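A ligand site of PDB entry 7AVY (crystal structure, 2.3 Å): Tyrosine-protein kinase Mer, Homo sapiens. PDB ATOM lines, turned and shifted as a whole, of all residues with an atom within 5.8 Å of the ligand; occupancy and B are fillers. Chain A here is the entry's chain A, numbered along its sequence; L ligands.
N of Met 106 sits at hydrogen-bond distance from N3 of the ligand (2.9 Å).
An oxygen (O3) of the ligand sits at hydrogen-bond distance from the backbone NH (N) of Asp 173 (3.3 Å).
N of Ala 49 is in hydrogen-bond range of O of Leu 103, at 3.0 Å.
The side-chain carboxylate (OD1) of Asp 173 is in salt-bridge range of the side-chain amino group (NZ) of Lys 51 (2.9 Å).
The backbone NH (N) of Leu 25 sits at hydrogen-bond distance from the backbone carbonyl oxygen (O) of Val 33 (2.8 Å).
The backbone NH (N) of Lys 51 lies within hydrogen-bond range of the backbone carbonyl oxygen (O) of Val 101, 2.9 Å away.
The side-chain carboxylate (OD1) of Asp 110 sits at hydrogen-bond distance from the side-chain hydroxyl (OG1) of Thr 113 (2.6 Å).
O of Gly 26 sits at hydrogen-bond distance from N of Val 33 (2.9 Å).
Leu 25 touches the ligand (O to C9, 3.4 Å).
CA of Gly 26 touches C9 of the ligand, 3.9 Å away.
Val 33 touches the ligand (CG1 to N4, 3.96 Å).
Ala 49 touches the ligand.
CB of Lys 51 touches N6 of the ligand, at 3.8 Å.
CD1 of Ile 82 touches C22 of the ligand (3.96 Å).
Leu 103 touches the ligand.
Pro 104 touches the ligand.
Phe 105 touches the ligand (C to N3, 3.9 Å).
Asp 110 touches the ligand (OD1 to C7, 3.9 Å).
OG1 of Thr 113 touches C7 of the ligand, at 3.96 Å.
Met 162 touches the ligand.
CB of Ala 172 touches N5 of the ligand, 3.4 Å away.
Phe 174 touches the ligand.
CD1 of Leu 176 touches C24 of the ligand, at 3.9 Å.
Within 4 Å of the ligand: Leu 25, Gly 26, Val 33, Ala 49, Lys 51, Ile 82, Leu 103, Pro 104, Phe 105, Met 106, Asp 110, Thr 113, Met 162, Ala 172, Asp 173, Phe 174 and Leu 176.
The nearest printed residue that does not touch the ligand is Gly 109 (4.1 Å).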
ATOM      1  N   LEU A  25      14.330  19.650  -1.332  1.00  0.00           N
ATOM      2  CA  LEU A  25      15.273  19.586  -2.445  1.00  0.00           C
ATOM      3  C   LEU A  25      16.097  18.315  -2.329  1.00  0.00           C
ATOM      4  O   LEU A  25      16.262  17.625  -3.331  1.00  0.00           O
ATOM      5  CB  LEU A  25      16.145  20.848  -2.539  1.00  0.00           C
ATOM      6  CG  LEU A  25      15.339  22.174  -2.646  1.00  0.00           C
ATOM      7  CD1 LEU A  25      16.201  23.360  -2.319  1.00  0.00           C
ATOM      8  CD2 LEU A  25      14.701  22.337  -4.012  1.00  0.00           C
ATOM      9  N   GLY A  26      16.526  17.962  -1.106  1.00  0.00           N
ATOM     10  CA  GLY A  26      17.318  16.764  -0.843  1.00  0.00           C
ATOM     11  C   GLY A  26      17.394  16.320   0.603  1.00  0.00           C
ATOM     12  O   GLY A  26      17.380  17.158   1.507  1.00  0.00           O
ATOM     13  N   VAL A  33      17.568  19.685   2.917  1.00  0.00           N
ATOM     14  CA  VAL A  33      17.557  20.976   2.206  1.00  0.00           C
ATOM     15  C   VAL A  33      16.147  21.123   1.649  1.00  0.00           C
ATOM     16  O   VAL A  33      15.600  20.182   1.065  1.00  0.00           O
ATOM     17  CB  VAL A  33      18.669  21.122   1.114  1.00  0.00           C
ATOM     18  CG1 VAL A  33      18.648  22.513   0.486  1.00  0.00           C
ATOM     19  CG2 VAL A  33      20.056  20.838   1.683  1.00  0.00           C
ATOM     20  N   ALA A  49      16.535  28.967   0.522  1.00  0.00           N
ATOM     21  CA  ALA A  49      16.980  27.598   0.664  1.00  0.00           C
ATOM     22  C   ALA A  49      17.247  27.373   2.148  1.00  0.00           C
ATOM     23  O   ALA A  49      17.942  28.165   2.790  1.00  0.00           O
ATOM     24  CB  ALA A  49      18.259  27.399  -0.118  1.00  0.00           C
ATOM     25  N   LYS A  51      18.598  24.803   5.199  1.00  0.00           N
ATOM     26  CA  LYS A  51      19.342  23.607   5.593  1.00  0.00           C
ATOM     27  C   LYS A  51      19.183  23.281   7.082  1.00  0.00           C
ATOM     28  O   LYS A  51      19.732  23.988   7.925  1.00  0.00           O
ATOM     29  CB  LYS A  51      20.817  23.635   5.194  1.00  0.00           C
ATOM     30  CG  LYS A  51      21.337  22.231   4.930  1.00  0.00           C
ATOM     31  CD  LYS A  51      22.641  21.911   5.620  1.00  0.00           C
ATOM     32  CE  LYS A  51      23.016  20.481   5.282  1.00  0.00           C
ATOM     33  NZ  LYS A  51      24.477  20.246   5.351  1.00  0.00           N
ATOM     34  N   MET A  53      19.640  20.892  10.493  1.00  0.00           N
ATOM     35  CA  MET A  53      20.620  20.011  11.122  1.00  0.00           C
ATOM     36  C   MET A  53      20.088  19.648  12.489  1.00  0.00           C
ATOM     37  O   MET A  53      19.151  20.289  12.952  1.00  0.00           O
ATOM     38  CB  MET A  53      21.941  20.761  11.302  1.00  0.00           C
ATOM     39  CG  MET A  53      22.468  21.392  10.062  1.00  0.00           C
ATOM     40  SD  MET A  53      23.561  22.722  10.525  1.00  0.00           S
ATOM     41  CE  MET A  53      24.993  21.767  11.041  1.00  0.00           C
ATOM     42  N   PHE A  66      28.348  27.008  17.612  1.00  0.00           N
ATOM     43  CA  PHE A  66      27.707  26.915  16.306  1.00  0.00           C
ATOM     44  C   PHE A  66      27.251  28.325  15.900  1.00  0.00           C
ATOM     45  O   PHE A  66      27.381  28.681  14.727  1.00  0.00           O
ATOM     46  CB  PHE A  66      26.504  25.943  16.355  1.00  0.00           C
ATOM     47  CG  PHE A  66      25.736  25.854  15.054  1.00  0.00           C
ATOM     48  CD1 PHE A  66      24.678  26.717  14.795  1.00  0.00           C
ATOM     49  CD2 PHE A  66      26.082  24.920  14.096  1.00  0.00           C
ATOM     50  CE1 PHE A  66      24.001  26.664  13.575  1.00  0.00           C
ATOM     51  CE2 PHE A  66      25.387  24.862  12.879  1.00  0.00           C
ATOM     52  CZ  PHE A  66      24.343  25.722  12.637  1.00  0.00           C
ATOM     53  N   MET A  73      30.312  33.368   9.081  1.00  0.00           N
ATOM     54  CA  MET A  73      29.828  33.157   7.711  1.00  0.00           C
ATOM     55  C   MET A  73      28.877  34.267   7.222  1.00  0.00           C
ATOM     56  O   MET A  73      28.924  34.610   6.037  1.00  0.00           O
ATOM     57  CB  MET A  73      29.180  31.785   7.564  1.00  0.00           C
ATOM     58  CG  MET A  73      30.063  30.626   7.962  1.00  0.00           C
ATOM     59  SD  MET A  73      29.099  29.083   8.006  1.00  0.00           S
ATOM     60  CE  MET A  73      30.136  28.076   9.057  1.00  0.00           C
ATOM     61  N   ILE A  82      28.852  31.587  -1.047  1.00  0.00           N
ATOM     62  CA  ILE A  82      27.400  31.699  -0.766  1.00  0.00           C
ATOM     63  C   ILE A  82      27.098  32.677   0.416  1.00  0.00           C
ATOM     64  O   ILE A  82      27.791  32.645   1.448  1.00  0.00           O
ATOM     65  CB  ILE A  82      26.682  30.323  -0.585  1.00  0.00           C
ATOM     66  CG1 ILE A  82      25.154  30.459  -0.855  1.00  0.00           C
ATOM     67  CG2 ILE A  82      26.955  29.692   0.799  1.00  0.00           C
ATOM     68  CD1 ILE A  82      24.436  29.160  -1.403  1.00  0.00           C
ATOM     69  N   LEU A  84      25.084  33.770   3.677  1.00  0.00           N
ATOM     70  CA  LEU A  84      24.299  33.198   4.768  1.00  0.00           C
ATOM     71  C   LEU A  84      23.418  34.324   5.325  1.00  0.00           C
ATOM     72  O   LEU A  84      23.934  35.276   5.921  1.00  0.00           O
ATOM     73  CB  LEU A  84      25.270  32.642   5.841  1.00  0.00           C
ATOM     74  CG  LEU A  84      24.677  31.858   7.015  1.00  0.00           C
ATOM     75  CD1 LEU A  84      25.609  30.752   7.414  1.00  0.00           C
ATOM     76  CD2 LEU A  84      24.478  32.743   8.219  1.00  0.00           C
ATOM     77  N   VAL A 101      19.701  26.849   8.863  1.00  0.00           N
ATOM     78  CA  VAL A 101      20.526  27.851   8.187  1.00  0.00           C
ATOM     79  C   VAL A 101      19.782  28.275   6.910  1.00  0.00           C
ATOM     80  O   VAL A 101      19.241  27.442   6.192  1.00  0.00           O
ATOM     81  CB  VAL A 101      21.955  27.314   7.948  1.00  0.00           C
ATOM     82  CG1 VAL A 101      22.843  28.359   7.277  1.00  0.00           C
ATOM     83  CG2 VAL A 101      22.585  26.833   9.263  1.00  0.00           C
ATOM     84  N   LEU A 103      19.831  30.537   3.421  1.00  0.00           N
ATOM     85  CA  LEU A 103      20.661  31.006   2.311  1.00  0.00           C
ATOM     86  C   LEU A 103      19.735  31.499   1.167  1.00  0.00           C
ATOM     87  O   LEU A 103      18.564  31.099   1.157  1.00  0.00           O
ATOM     88  CB  LEU A 103      21.528  29.820   1.764  1.00  0.00           C
ATOM     89  CG  LEU A 103      22.200  28.953   2.813  1.00  0.00           C
ATOM     90  CD1 LEU A 103      21.544  27.603   2.920  1.00  0.00           C
ATOM     91  CD2 LEU A 103      23.693  28.885   2.586  1.00  0.00           C
ATOM     92  N   PRO A 104      20.217  32.263   0.146  1.00  0.00           N
ATOM     93  CA  PRO A 104      19.328  32.589  -0.989  1.00  0.00           C
ATOM     94  C   PRO A 104      19.034  31.316  -1.808  1.00  0.00           C
ATOM     95  O   PRO A 104      19.911  30.460  -1.915  1.00  0.00           O
ATOM     96  CB  PRO A 104      20.185  33.530  -1.851  1.00  0.00           C
ATOM     97  CG  PRO A 104      21.375  33.875  -1.037  1.00  0.00           C
ATOM     98  CD  PRO A 104      21.582  32.781  -0.081  1.00  0.00           C
ATOM     99  N   PHE A 105      17.811  31.203  -2.369  1.00  0.00           N
ATOM    100  CA  PHE A 105      17.402  30.098  -3.217  1.00  0.00           C
ATOM    101  C   PHE A 105      18.113  30.244  -4.564  1.00  0.00           C
ATOM    102  O   PHE A 105      18.037  31.308  -5.178  1.00  0.00           O
ATOM    103  CB  PHE A 105      15.863  30.064  -3.402  1.00  0.00           C
ATOM    104  CG  PHE A 105      15.367  29.000  -4.365  1.00  0.00           C
ATOM    105  CD1 PHE A 105      15.331  27.662  -3.997  1.00  0.00           C
ATOM    106  CD2 PHE A 105      14.949  29.336  -5.660  1.00  0.00           C
ATOM    107  CE1 PHE A 105      14.890  26.682  -4.889  1.00  0.00           C
ATOM    108  CE2 PHE A 105      14.517  28.359  -6.554  1.00  0.00           C
ATOM    109  CZ  PHE A 105      14.504  27.030  -6.168  1.00  0.00           C
ATOM    110  N   MET A 106      18.838  29.178  -4.976  1.00  0.00           N
ATOM    111  CA  MET A 106      19.626  29.090  -6.213  1.00  0.00           C
ATOM    112  C   MET A 106      18.860  28.247  -7.268  1.00  0.00           C
ATOM    113  O   MET A 106      18.955  27.004  -7.275  1.00  0.00           O
ATOM    114  CB  MET A 106      21.005  28.490  -5.898  1.00  0.00           C
ATOM    115  CG  MET A 106      22.178  29.410  -6.167  1.00  0.00           C
ATOM    116  SD  MET A 106      22.357  30.870  -5.138  1.00  0.00           S
ATOM    117  CE  MET A 106      21.604  32.018  -6.111  1.00  0.00           C
ATOM    118  N   LYS A 107      18.089  28.944  -8.154  1.00  0.00           N
ATOM    119  CA  LYS A 107      17.257  28.319  -9.196  1.00  0.00           C
ATOM    120  C   LYS A 107      18.040  27.448 -10.204  1.00  0.00           C
ATOM    121  O   LYS A 107      17.489  26.447 -10.674  1.00  0.00           O
ATOM    122  CB  LYS A 107      16.383  29.359  -9.918  1.00  0.00           C
ATOM    123  CG  LYS A 107      17.142  30.368 -10.757  1.00  0.00           C
ATOM    124  CD  LYS A 107      16.225  31.425 -11.356  1.00  0.00           C
ATOM    125  CE  LYS A 107      16.837  31.954 -12.625  1.00  0.00           C
ATOM    126  NZ  LYS A 107      16.052  33.093 -13.195  1.00  0.00           N
ATOM    127  N   TYR A 108      19.293  27.802 -10.529  1.00  0.00           N
ATOM    128  CA  TYR A 108      20.045  26.979 -11.473  1.00  0.00           C
ATOM    129  C   TYR A 108      20.617  25.701 -10.838  1.00  0.00           C
ATOM    130  O   TYR A 108      21.068  24.829 -11.561  1.00  0.00           O
ATOM    131  CB  TYR A 108      21.118  27.790 -12.226  1.00  0.00           C
ATOM    132  CG  TYR A 108      20.529  28.822 -13.168  1.00  0.00           C
ATOM    133  CD1 TYR A 108      19.511  28.484 -14.061  1.00  0.00           C
ATOM    134  CD2 TYR A 108      21.040  30.116 -13.229  1.00  0.00           C
ATOM    135  CE1 TYR A 108      18.950  29.433 -14.926  1.00  0.00           C
ATOM    136  CE2 TYR A 108      20.507  31.065 -14.113  1.00  0.00           C
ATOM    137  CZ  TYR A 108      19.471  30.717 -14.950  1.00  0.00           C
ATOM    138  OH  TYR A 108      18.947  31.636 -15.833  1.00  0.00           O
ATOM    139  N   GLY A 109      20.534  25.602  -9.503  1.00  0.00           N
ATOM    140  CA  GLY A 109      20.949  24.449  -8.695  1.00  0.00           C
ATOM    141  C   GLY A 109      22.453  24.246  -8.532  1.00  0.00           C
ATOM    142  O   GLY A 109      23.240  25.165  -8.781  1.00  0.00           O
ATOM    143  N   ASP A 110      22.842  23.027  -8.099  1.00  0.00           N
ATOM    144  CA  ASP A 110      24.257  22.709  -7.900  1.00  0.00           C
ATOM    145  C   ASP A 110      24.994  22.476  -9.216  1.00  0.00           C
ATOM    146  O   ASP A 110      24.381  22.173 -10.254  1.00  0.00           O
ATOM    147  CB  ASP A 110      24.454  21.530  -6.953  1.00  0.00           C
ATOM    148  CG  ASP A 110      24.052  20.196  -7.555  1.00  0.00           C
ATOM    149  OD1 ASP A 110      22.844  20.000  -7.788  1.00  0.00           O
ATOM    150  OD2 ASP A 110      24.931  19.359  -7.786  1.00  0.00           O
ATOM    151  N   THR A 113      24.964  18.490 -10.720  1.00  0.00           N
ATOM    152  CA  THR A 113      23.798  18.164 -11.546  1.00  0.00           C
ATOM    153  C   THR A 113      23.859  18.886 -12.933  1.00  0.00           C
ATOM    154  O   THR A 113      23.516  18.274 -13.936  1.00  0.00           O
ATOM    155  CB  THR A 113      22.489  18.505 -10.825  1.00  0.00           C
ATOM    156  OG1 THR A 113      22.537  18.045  -9.483  1.00  0.00           O
ATOM    157  CG2 THR A 113      21.263  17.918 -11.513  1.00  0.00           C
ATOM    158  N   MET A 162      27.263  26.029  -5.951  1.00  0.00           N
ATOM    159  CA  MET A 162      25.972  26.471  -6.515  1.00  0.00           C
ATOM    160  C   MET A 162      26.191  27.448  -7.663  1.00  0.00           C
ATOM    161  O   MET A 162      27.108  28.280  -7.596  1.00  0.00           O
ATOM    162  CB  MET A 162      25.108  27.186  -5.441  1.00  0.00           C
ATOM    163  CG  MET A 162      24.649  26.291  -4.269  1.00  0.00           C
ATOM    164  SD  MET A 162      23.555  24.905  -4.758  1.00  0.00           S
ATOM    165  CE  MET A 162      24.021  23.700  -3.560  1.00  0.00           C
ATOM    166  N   ALA A 172      29.527  26.560  -1.310  1.00  0.00           N
ATOM    167  CA  ALA A 172      28.450  26.435  -0.328  1.00  0.00           C
ATOM    168  C   ALA A 172      28.597  25.186   0.538  1.00  0.00           C
ATOM    169  O   ALA A 172      29.605  24.482   0.446  1.00  0.00           O
ATOM    170  CB  ALA A 172      27.119  26.383  -1.079  1.00  0.00           C
ATOM    171  N   ASP A 173      27.561  24.908   1.360  1.00  0.00           N
ATOM    172  CA  ASP A 173      27.410  23.724   2.198  1.00  0.00           C
ATOM    173  C   ASP A 173      28.681  23.294   2.943  1.00  0.00           C
ATOM    174  O   ASP A 173      29.148  22.165   2.789  1.00  0.00           O
ATOM    175  CB  ASP A 173      26.836  22.564   1.348  1.00  0.00           C
ATOM    176  CG  ASP A 173      25.955  21.583   2.088  1.00  0.00           C
ATOM    177  OD1 ASP A 173      26.076  21.474   3.322  1.00  0.00           O
ATOM    178  OD2 ASP A 173      25.152  20.902   1.430  1.00  0.00           O
ATOM    179  N   PHE A 174      29.217  24.214   3.749  1.00  0.00           N
ATOM    180  CA  PHE A 174      30.432  23.999   4.556  1.00  0.00           C
ATOM    181  C   PHE A 174      30.176  22.929   5.604  1.00  0.00           C
ATOM    182  O   PHE A 174      29.061  22.823   6.108  1.00  0.00           O
ATOM    183  CB  PHE A 174      30.853  25.303   5.263  1.00  0.00           C
ATOM    184  CG  PHE A 174      30.721  26.549   4.413  1.00  0.00           C
ATOM    185  CD1 PHE A 174      31.625  26.820   3.400  1.00  0.00           C
ATOM    186  CD2 PHE A 174      29.676  27.441   4.630  1.00  0.00           C
ATOM    187  CE1 PHE A 174      31.488  27.964   2.599  1.00  0.00           C
ATOM    188  CE2 PHE A 174      29.540  28.586   3.829  1.00  0.00           C
ATOM    189  CZ  PHE A 174      30.441  28.832   2.821  1.00  0.00           C
ATOM    190  N   GLY A 175      31.218  22.157   5.902  1.00  0.00           N
ATOM    191  CA  GLY A 175      31.214  21.107   6.918  1.00  0.00           C
ATOM    192  C   GLY A 175      31.594  21.654   8.278  1.00  0.00           C
ATOM    193  O   GLY A 175      32.053  22.797   8.383  1.00  0.00           O
ATOM    194  N   LEU A 176      31.392  20.858   9.341  1.00  0.00           N
ATOM    195  CA  LEU A 176      31.698  21.299  10.715  1.00  0.00           C
ATOM    196  C   LEU A 176      32.495  20.264  11.535  1.00  0.00           C
ATOM    197  O   LEU A 176      32.690  19.127  11.068  1.00  0.00           O
ATOM    198  CB  LEU A 176      30.407  21.737  11.446  1.00  0.00           C
ATOM    199  CG  LEU A 176      29.691  22.973  10.883  1.00  0.00           C
ATOM    200  CD1 LEU A 176      28.478  22.585  10.053  1.00  0.00           C
ATOM    201  CD2 LEU A 176      29.311  23.948  11.990  1.00  0.00           C
HETATM  202  C1  LIG L   1      18.698  23.748  -5.111  1.00  0.00           C
HETATM  203  C2  LIG L   1      18.807  25.078  -4.816  1.00  0.00           C
HETATM  204  C3  LIG L   1      19.615  25.507  -3.744  1.00  0.00           C
HETATM  205  C4  LIG L   1      19.618  20.434  -3.834  1.00  0.00           C
HETATM  206  C5  LIG L   1      19.896  19.167  -4.637  1.00  0.00           C
HETATM  207  C6  LIG L   1      19.116  19.072  -5.959  1.00  0.00           C
HETATM  208  C7  LIG L   1      19.737  17.883  -6.686  1.00  0.00           C
HETATM  209  C8  LIG L   1      20.224  16.752  -4.552  1.00  0.00           C
HETATM  210  C9  LIG L   1      19.625  17.925  -3.793  1.00  0.00           C
HETATM  211  C10 LIG L   1      21.120  25.076  -1.897  1.00  0.00           C
HETATM  212  C11 LIG L   1      20.471  27.187  -2.468  1.00  0.00           C
HETATM  213  C12 LIG L   1      22.625  24.574   0.007  1.00  0.00           C
HETATM  214  C13 LIG L   1      22.441  24.018   1.269  1.00  0.00           C
HETATM  215  C14 LIG L   1      24.704  25.162   4.489  1.00  0.00           C
HETATM  216  C15 LIG L   1      25.807  25.742   5.348  1.00  0.00           C
HETATM  217  C16 LIG L   1      25.676  25.392   6.833  1.00  0.00           C
HETATM  218  C17 LIG L   1      26.915  25.350   7.680  1.00  0.00           C
HETATM  219  C18 LIG L   1      17.277  24.145  -7.002  1.00  0.00           C
HETATM  220  O1  LIG L   1      17.936  23.227  -6.134  1.00  0.00           O
HETATM  221  C19 LIG L   1      19.402  22.785  -4.343  1.00  0.00           C
HETATM  222  O2  LIG L   1      19.213  21.481  -4.738  1.00  0.00           O
HETATM  223  N1  LIG L   1      19.672  16.601  -5.919  1.00  0.00           N
HETATM  224  C20 LIG L   1      20.193  23.176  -3.298  1.00  0.00           C
HETATM  225  C21 LIG L   1      20.318  24.544  -2.976  1.00  0.00           C
HETATM  226  N2  LIG L   1      21.186  26.398  -1.667  1.00  0.00           N
HETATM  227  N3  LIG L   1      19.690  26.854  -3.489  1.00  0.00           N
HETATM  228  N4  LIG L   1      21.838  24.229  -1.111  1.00  0.00           N
HETATM  229  C22 LIG L   1      23.643  25.522  -0.051  1.00  0.00           C
HETATM  230  N5  LIG L   1      24.415  25.875   0.999  1.00  0.00           N
HETATM  231  C23 LIG L   1      24.115  25.253   2.125  1.00  0.00           C
HETATM  232  N6  LIG L   1      23.177  24.332   2.351  1.00  0.00           N
HETATM  233  O3  LIG L   1      24.896  25.628   3.147  1.00  0.00           O
HETATM  234  C24 LIG L   1      26.207  24.078   7.319  1.00  0.00           C
